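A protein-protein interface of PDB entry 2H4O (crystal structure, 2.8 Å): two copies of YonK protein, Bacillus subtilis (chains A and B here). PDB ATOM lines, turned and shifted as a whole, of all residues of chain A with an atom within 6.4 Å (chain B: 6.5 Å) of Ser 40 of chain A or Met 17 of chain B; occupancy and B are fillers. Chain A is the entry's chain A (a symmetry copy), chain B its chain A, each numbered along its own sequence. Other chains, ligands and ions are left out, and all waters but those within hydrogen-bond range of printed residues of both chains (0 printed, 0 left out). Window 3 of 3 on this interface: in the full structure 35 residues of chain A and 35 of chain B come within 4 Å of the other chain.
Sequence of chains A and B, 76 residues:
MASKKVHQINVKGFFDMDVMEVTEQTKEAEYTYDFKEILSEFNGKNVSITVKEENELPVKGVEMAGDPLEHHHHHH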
ATOM      1  N   MET A  20      -1.595  26.715 -28.814  1.00  0.00           N
ATOM      2  CA  MET A  20      -0.625  25.653 -28.593  1.00  0.00           C
ATOM      3  C   MET A  20      -1.143  24.258 -28.954  1.00  0.00           C
ATOM      4  O   MET A  20      -1.073  23.323 -28.153  1.00  0.00           O
ATOM      5  CB  MET A  20      -0.146  25.675 -27.144  1.00  0.00           C
ATOM      6  CG  MET A  20       1.053  26.588 -26.910  1.00  0.00           C
ATOM      7  SD  MET A  20       2.763  25.920 -27.628  1.00  0.00           S
ATOM      8  CE  MET A  20       3.403  24.944 -26.093  1.00  0.00           C
ATOM      9  N   PHE A  35      -0.197  20.390 -28.023  1.00  0.00           N
ATOM     10  CA  PHE A  35       1.239  20.402 -27.891  1.00  0.00           C
ATOM     11  C   PHE A  35       1.676  20.730 -26.474  1.00  0.00           C
ATOM     12  O   PHE A  35       2.738  20.273 -26.031  1.00  0.00           O
ATOM     13  CB  PHE A  35       1.797  21.401 -28.888  1.00  0.00           C
ATOM     14  CG  PHE A  35       3.215  21.187 -29.203  1.00  0.00           C
ATOM     15  CD1 PHE A  35       3.688  19.907 -29.441  1.00  0.00           C
ATOM     16  CD2 PHE A  35       4.092  22.260 -29.278  1.00  0.00           C
ATOM     17  CE1 PHE A  35       5.007  19.697 -29.742  1.00  0.00           C
ATOM     18  CE2 PHE A  35       5.424  22.058 -29.582  1.00  0.00           C
ATOM     19  CZ  PHE A  35       5.884  20.769 -29.818  1.00  0.00           C
ATOM     20  N   LYS A  36       0.844  21.501 -25.768  1.00  0.00           N
ATOM     21  CA  LYS A  36       1.120  21.890 -24.387  1.00  0.00           C
ATOM     22  C   LYS A  36       1.228  20.644 -23.486  1.00  0.00           C
ATOM     23  O   LYS A  36       2.237  20.420 -22.818  1.00  0.00           O
ATOM     24  CB  LYS A  36       0.005  22.830 -23.887  1.00  0.00           C
ATOM     25  CG  LYS A  36       0.349  23.650 -22.626  1.00  0.00           C
ATOM     26  CD  LYS A  36      -0.850  24.536 -22.172  1.00  0.00           C
ATOM     27  CE  LYS A  36      -0.435  25.780 -21.294  1.00  0.00           C
ATOM     28  NZ  LYS A  36       0.356  25.469 -20.052  1.00  0.00           N
ATOM     29  N   GLU A  37       0.185  19.830 -23.484  1.00  0.00           N
ATOM     30  CA  GLU A  37       0.183  18.621 -22.673  1.00  0.00           C
ATOM     31  C   GLU A  37       1.339  17.720 -23.065  1.00  0.00           C
ATOM     32  O   GLU A  37       2.060  17.217 -22.206  1.00  0.00           O
ATOM     33  CB  GLU A  37      -1.125  17.854 -22.847  1.00  0.00           C
ATOM     34  CG  GLU A  37      -1.655  17.299 -21.559  1.00  0.00           C
ATOM     35  CD  GLU A  37      -1.699  18.353 -20.457  1.00  0.00           C
ATOM     36  OE1 GLU A  37      -0.825  18.304 -19.555  1.00  0.00           O
ATOM     37  OE2 GLU A  37      -2.595  19.239 -20.508  1.00  0.00           O
ATOM     38  N   ILE A  38       1.495  17.498 -24.367  1.00  0.00           N
ATOM     39  CA  ILE A  38       2.589  16.673 -24.878  1.00  0.00           C
ATOM     40  C   ILE A  38       3.954  17.198 -24.383  1.00  0.00           C
ATOM     41  O   ILE A  38       4.757  16.461 -23.780  1.00  0.00           O
ATOM     42  CB  ILE A  38       2.588  16.669 -26.430  1.00  0.00           C
ATOM     43  CG1 ILE A  38       1.334  15.954 -26.958  1.00  0.00           C
ATOM     44  CG2 ILE A  38       3.858  16.004 -26.943  1.00  0.00           C
ATOM     45  CD1 ILE A  38       1.133  16.100 -28.422  1.00  0.00           C
ATOM     46  N   LEU A  39       4.194  18.486 -24.633  1.00  0.00           N
ATOM     47  CA  LEU A  39       5.431  19.128 -24.235  1.00  0.00           C
ATOM     48  C   LEU A  39       5.708  19.009 -22.766  1.00  0.00           C
ATOM     49  O   LEU A  39       6.836  18.851 -22.376  1.00  0.00           O
ATOM     50  CB  LEU A  39       5.392  20.593 -24.636  1.00  0.00           C
ATOM     51  CG  LEU A  39       6.532  21.147 -25.479  1.00  0.00           C
ATOM     52  CD1 LEU A  39       6.807  20.219 -26.650  1.00  0.00           C
ATOM     53  CD2 LEU A  39       6.150  22.530 -25.954  1.00  0.00           C
ATOM     54  N   SER A  40       4.676  19.085 -21.943  1.00  0.00           N
ATOM     55  CA  SER A  40       4.866  19.007 -20.500  1.00  0.00           C
ATOM     56  C   SER A  40       5.380  17.676 -20.005  1.00  0.00           C
ATOM     57  O   SER A  40       6.010  17.608 -18.966  1.00  0.00           O
ATOM     58  CB  SER A  40       3.571  19.323 -19.782  1.00  0.00           C
ATOM     59  OG  SER A  40       2.640  18.301 -19.998  1.00  0.00           O
ATOM     60  N   GLU A  41       5.102  16.614 -20.744  1.00  0.00           N
ATOM     61  CA  GLU A  41       5.532  15.289 -20.352  1.00  0.00           C
ATOM     62  C   GLU A  41       7.058  15.261 -20.324  1.00  0.00           C
ATOM     63  O   GLU A  41       7.688  14.373 -19.747  1.00  0.00           O
ATOM     64  CB  GLU A  41       4.978  14.291 -21.368  1.00  0.00           C
ATOM     65  CG  GLU A  41       5.082  12.799 -21.023  1.00  0.00           C
ATOM     66  CD  GLU A  41       4.354  11.915 -22.045  1.00  0.00           C
ATOM     67  OE1 GLU A  41       4.583  10.680 -22.050  1.00  0.00           O
ATOM     68  OE2 GLU A  41       3.548  12.455 -22.846  1.00  0.00           O
ATOM     69  N   PHE A  42       7.661  16.262 -20.943  1.00  0.00           N
ATOM     70  CA  PHE A  42       9.118  16.324 -21.020  1.00  0.00           C
ATOM     71  C   PHE A  42       9.759  17.450 -20.201  1.00  0.00           C
ATOM     72  O   PHE A  42      10.986  17.522 -20.084  1.00  0.00           O
ATOM     73  CB  PHE A  42       9.566  16.440 -22.487  1.00  0.00           C
ATOM     74  CG  PHE A  42       9.207  15.247 -23.338  1.00  0.00           C
ATOM     75  CD1 PHE A  42       8.119  15.290 -24.206  1.00  0.00           C
ATOM     76  CD2 PHE A  42       9.980  14.092 -23.294  1.00  0.00           C
ATOM     77  CE1 PHE A  42       7.813  14.213 -25.016  1.00  0.00           C
ATOM     78  CE2 PHE A  42       9.679  13.001 -24.104  1.00  0.00           C
ATOM     79  CZ  PHE A  42       8.594  13.065 -24.968  1.00  0.00           C
ATOM     80  N   ASN A  43       8.942  18.318 -19.624  1.00  0.00           N
ATOM     81  CA  ASN A  43       9.476  19.406 -18.825  1.00  0.00           C
ATOM     82  C   ASN A  43      10.344  18.931 -17.672  1.00  0.00           C
ATOM     83  O   ASN A  43       9.889  18.204 -16.808  1.00  0.00           O
ATOM     84  CB  ASN A  43       8.348  20.264 -18.271  1.00  0.00           C
ATOM     85  CG  ASN A  43       8.860  21.487 -17.536  1.00  0.00           C
ATOM     86  OD1 ASN A  43       9.584  22.301 -18.105  1.00  0.00           O
ATOM     87  ND2 ASN A  43       8.483  21.624 -16.272  1.00  0.00           N
ATOM     88  N   GLY A  44      11.601  19.354 -17.669  1.00  0.00           N
ATOM     89  CA  GLY A  44      12.509  18.969 -16.612  1.00  0.00           C
ATOM     90  C   GLY A  44      13.546  17.930 -16.977  1.00  0.00           C
ATOM     91  O   GLY A  44      14.178  17.355 -16.096  1.00  0.00           O
ATOM     92  N   PHE B  15      15.346  20.760 -20.866  1.00  0.00           N
ATOM     93  CA  PHE B  15      14.100  21.472 -21.117  1.00  0.00           C
ATOM     94  C   PHE B  15      13.319  21.968 -19.919  1.00  0.00           C
ATOM     95  O   PHE B  15      12.953  21.209 -19.034  1.00  0.00           O
ATOM     96  CB  PHE B  15      13.187  20.599 -21.959  1.00  0.00           C
ATOM     97  CG  PHE B  15      11.894  21.249 -22.314  1.00  0.00           C
ATOM     98  CD1 PHE B  15      11.877  22.504 -22.899  1.00  0.00           C
ATOM     99  CD2 PHE B  15      10.687  20.578 -22.146  1.00  0.00           C
ATOM    100  CE1 PHE B  15      10.675  23.084 -23.321  1.00  0.00           C
ATOM    101  CE2 PHE B  15       9.485  21.155 -22.570  1.00  0.00           C
ATOM    102  CZ  PHE B  15       9.489  22.413 -23.162  1.00  0.00           C
ATOM    103  N   ASP B  16      13.056  23.269 -19.919  1.00  0.00           N
ATOM    104  CA  ASP B  16      12.293  23.926 -18.868  1.00  0.00           C
ATOM    105  C   ASP B  16      11.146  24.657 -19.557  1.00  0.00           C
ATOM    106  O   ASP B  16      11.327  25.730 -20.148  1.00  0.00           O
ATOM    107  CB  ASP B  16      13.168  24.913 -18.106  1.00  0.00           C
ATOM    108  CG  ASP B  16      12.501  25.413 -16.838  1.00  0.00           C
ATOM    109  OD1 ASP B  16      11.513  26.183 -16.930  1.00  0.00           O
ATOM    110  OD2 ASP B  16      12.959  25.021 -15.747  1.00  0.00           O
ATOM    111  N   MET B  17       9.967  24.045 -19.475  1.00  0.00           N
ATOM    112  CA  MET B  17       8.773  24.552 -20.115  1.00  0.00           C
ATOM    113  C   MET B  17       8.129  25.707 -19.397  1.00  0.00           C
ATOM    114  O   MET B  17       7.257  26.370 -19.953  1.00  0.00           O
ATOM    115  CB  MET B  17       7.761  23.427 -20.262  1.00  0.00           C
ATOM    116  CG  MET B  17       6.536  23.825 -21.051  1.00  0.00           C
ATOM    117  SD  MET B  17       5.194  22.476 -20.946  1.00  0.00           S
ATOM    118  CE  MET B  17       5.151  22.223 -18.987  1.00  0.00           C
ATOM    119  N   ASP B  18       8.564  25.944 -18.162  1.00  0.00           N
ATOM    120  CA  ASP B  18       8.018  27.031 -17.341  1.00  0.00           C
ATOM    121  C   ASP B  18       8.495  28.354 -17.928  1.00  0.00           C
ATOM    122  O   ASP B  18       7.704  29.274 -18.147  1.00  0.00           O
ATOM    123  CB  ASP B  18       8.491  26.874 -15.894  1.00  0.00           C
ATOM    124  CG  ASP B  18       8.459  25.423 -15.428  1.00  0.00           C
ATOM    125  OD1 ASP B  18       7.369  24.810 -15.465  1.00  0.00           O
ATOM    126  OD2 ASP B  18       9.526  24.884 -15.036  1.00  0.00           O
ATOM    127  N   VAL B  19       9.795  28.428 -18.210  1.00  0.00           N
ATOM    128  CA  VAL B  19      10.391  29.618 -18.801  1.00  0.00           C
ATOM    129  C   VAL B  19      10.486  29.380 -20.300  1.00  0.00           C
ATOM    130  O   VAL B  19      10.933  30.241 -21.052  1.00  0.00           O
ATOM    131  CB  VAL B  19      11.800  29.853 -18.267  1.00  0.00           C
ATOM    132  CG1 VAL B  19      12.199  31.308 -18.489  1.00  0.00           C
ATOM    133  CG2 VAL B  19      11.862  29.487 -16.800  1.00  0.00           C
ATOM    134  N   MET B  20      10.061  28.191 -20.722  1.00  0.00           N
ATOM    135  CA  MET B  20      10.093  27.791 -22.120  1.00  0.00           C
ATOM    136  C   MET B  20      11.473  27.931 -22.771  1.00  0.00           C
ATOM    137  O   MET B  20      11.622  28.547 -23.828  1.00  0.00           O
ATOM    138  CB  MET B  20       9.058  28.581 -22.915  1.00  0.00           C
ATOM    139  CG  MET B  20       7.678  27.931 -22.936  1.00  0.00           C
ATOM    140  SD  MET B  20       7.534  26.317 -24.058  1.00  0.00           S
ATOM    141  CE  MET B  20       7.010  27.124 -25.728  1.00  0.00           C
ATOM    142  N   GLU B  21      12.476  27.330 -22.135  1.00  0.00           N
ATOM    143  CA  GLU B  21      13.843  27.373 -22.639  1.00  0.00           C
ATOM    144  C   GLU B  21      14.567  26.015 -22.618  1.00  0.00           C
ATOM    145  O   GLU B  21      14.371  25.182 -21.744  1.00  0.00           O
ATOM    146  CB  GLU B  21      14.669  28.370 -21.832  1.00  0.00           C
ATOM    147  CG  GLU B  21      14.041  29.747 -21.715  1.00  0.00           C
ATOM    148  CD  GLU B  21      14.915  30.725 -20.951  1.00  0.00           C
ATOM    149  OE1 GLU B  21      15.425  30.356 -19.865  1.00  0.00           O
ATOM    150  OE2 GLU B  21      15.082  31.869 -21.436  1.00  0.00           O
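Printed residues of chain B within 4 Å of Leu 39 of chain A: Phe 15 (3.5 Å) and Met 17 (3.9 Å). Of the printed residues of chain B, Gly 44 of chain A touches Phe 15 (2.7 Å). Of the printed residues of chain A, Phe 15 of chain B touches Leu 39, Phe 42, Asn 43 and Gly 44. Of the printed residues of chain A, Asp 16 of chain B touches Asn 43 (3.2 Å). Of chain A, only Leu 39 (3.9 Å), Ser 40 (3.4 Å) and Asn 43 (2.3 Å) come within 4 Å of Met 17 of chain B. The nearest residue of chain B that does not touch Ser 40 of chain A is Phe 15 of chain B (5.3 Å). The nearest residue of chain A that does not touch Met 17 of chain B is Lys 36 of chain A (4.1 Å). The nearest printed residue of chain B that does not touch Asn 43 of chain A is Val 19 of chain B (6.1 Å).
The side-chain hydroxyl (OG) of Ser 40 of chain A sits at hydrogen-bond distance from the backbone carbonyl oxygen (O) of Glu 37 of chain A (2.5 Å). The backbone NH (N) of Val 19 of chain B lies within hydrogen-bond range of the side-chain carboxylate (OD1) of Asp 16 of chain B, at 3.1 Å. OD1 of Asp 16 of chain B lies close to N of Asp 18 of chain B. The backbone carbonyl oxygen of Asp 16 of chain B is in hydrogen-bond range of the backbone NH of Glu 21 of chain B (2.8 Å).
Of the 11 printed residues of chain A, 5 touch a printed residue of chain B. Printed residues of chain A that touch a printed residue of chain B: Leu 39, Ser 40, Phe 42, Asn 43 and Gly 44. Hydrophobic or aromatic side chains of chain B within 4 Å of the printed part of chain A: Phe 15 and Met 17. Among the printed residues, 9 pairs touch across the chains. Among the printed residues, no Asp or Glu carboxylate lies within 4 Å of a Lys or Arg side-chain nitrogen of the other chain.
The side-chain amide oxygen (OD1) of Asn 43 of chain A sits close to the backbone NH (N) of Met 17 of chain B, at 2.3 Å. O of Phe 15 of chain B lies within hydrogen-bond range of N of Gly 44 of chain A. The side-chain sulfur (SD) of Met 17 of chain B sits close to the backbone NH (N) of Ser 40 of chain A (3.6 Å). The side-chain carboxylate (OD1) of Asp 18 of chain B sits at hydrogen-bond distance from the side-chain amide nitrogen (ND2) of Asn 43 of chain A (3.5 Å).
1 position is printed for both chains.
CE2 of Phe 15 of chain B touches O of Leu 39 of chain A, at 3.5 Å. Leu 39 of chain A touches Met 17 of chain B (C to SD, 3.9 Å). Phe 42 of chain A touches Phe 15 of chain B (O to CD2, 3.7 Å). Asn 43 of chain A touches Phe 15 of chain B (OD1 to O, 3.7 Å). OD1 of Asn 43 of chain A touches C of Asp 16 of chain B, at 3.2 Å.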
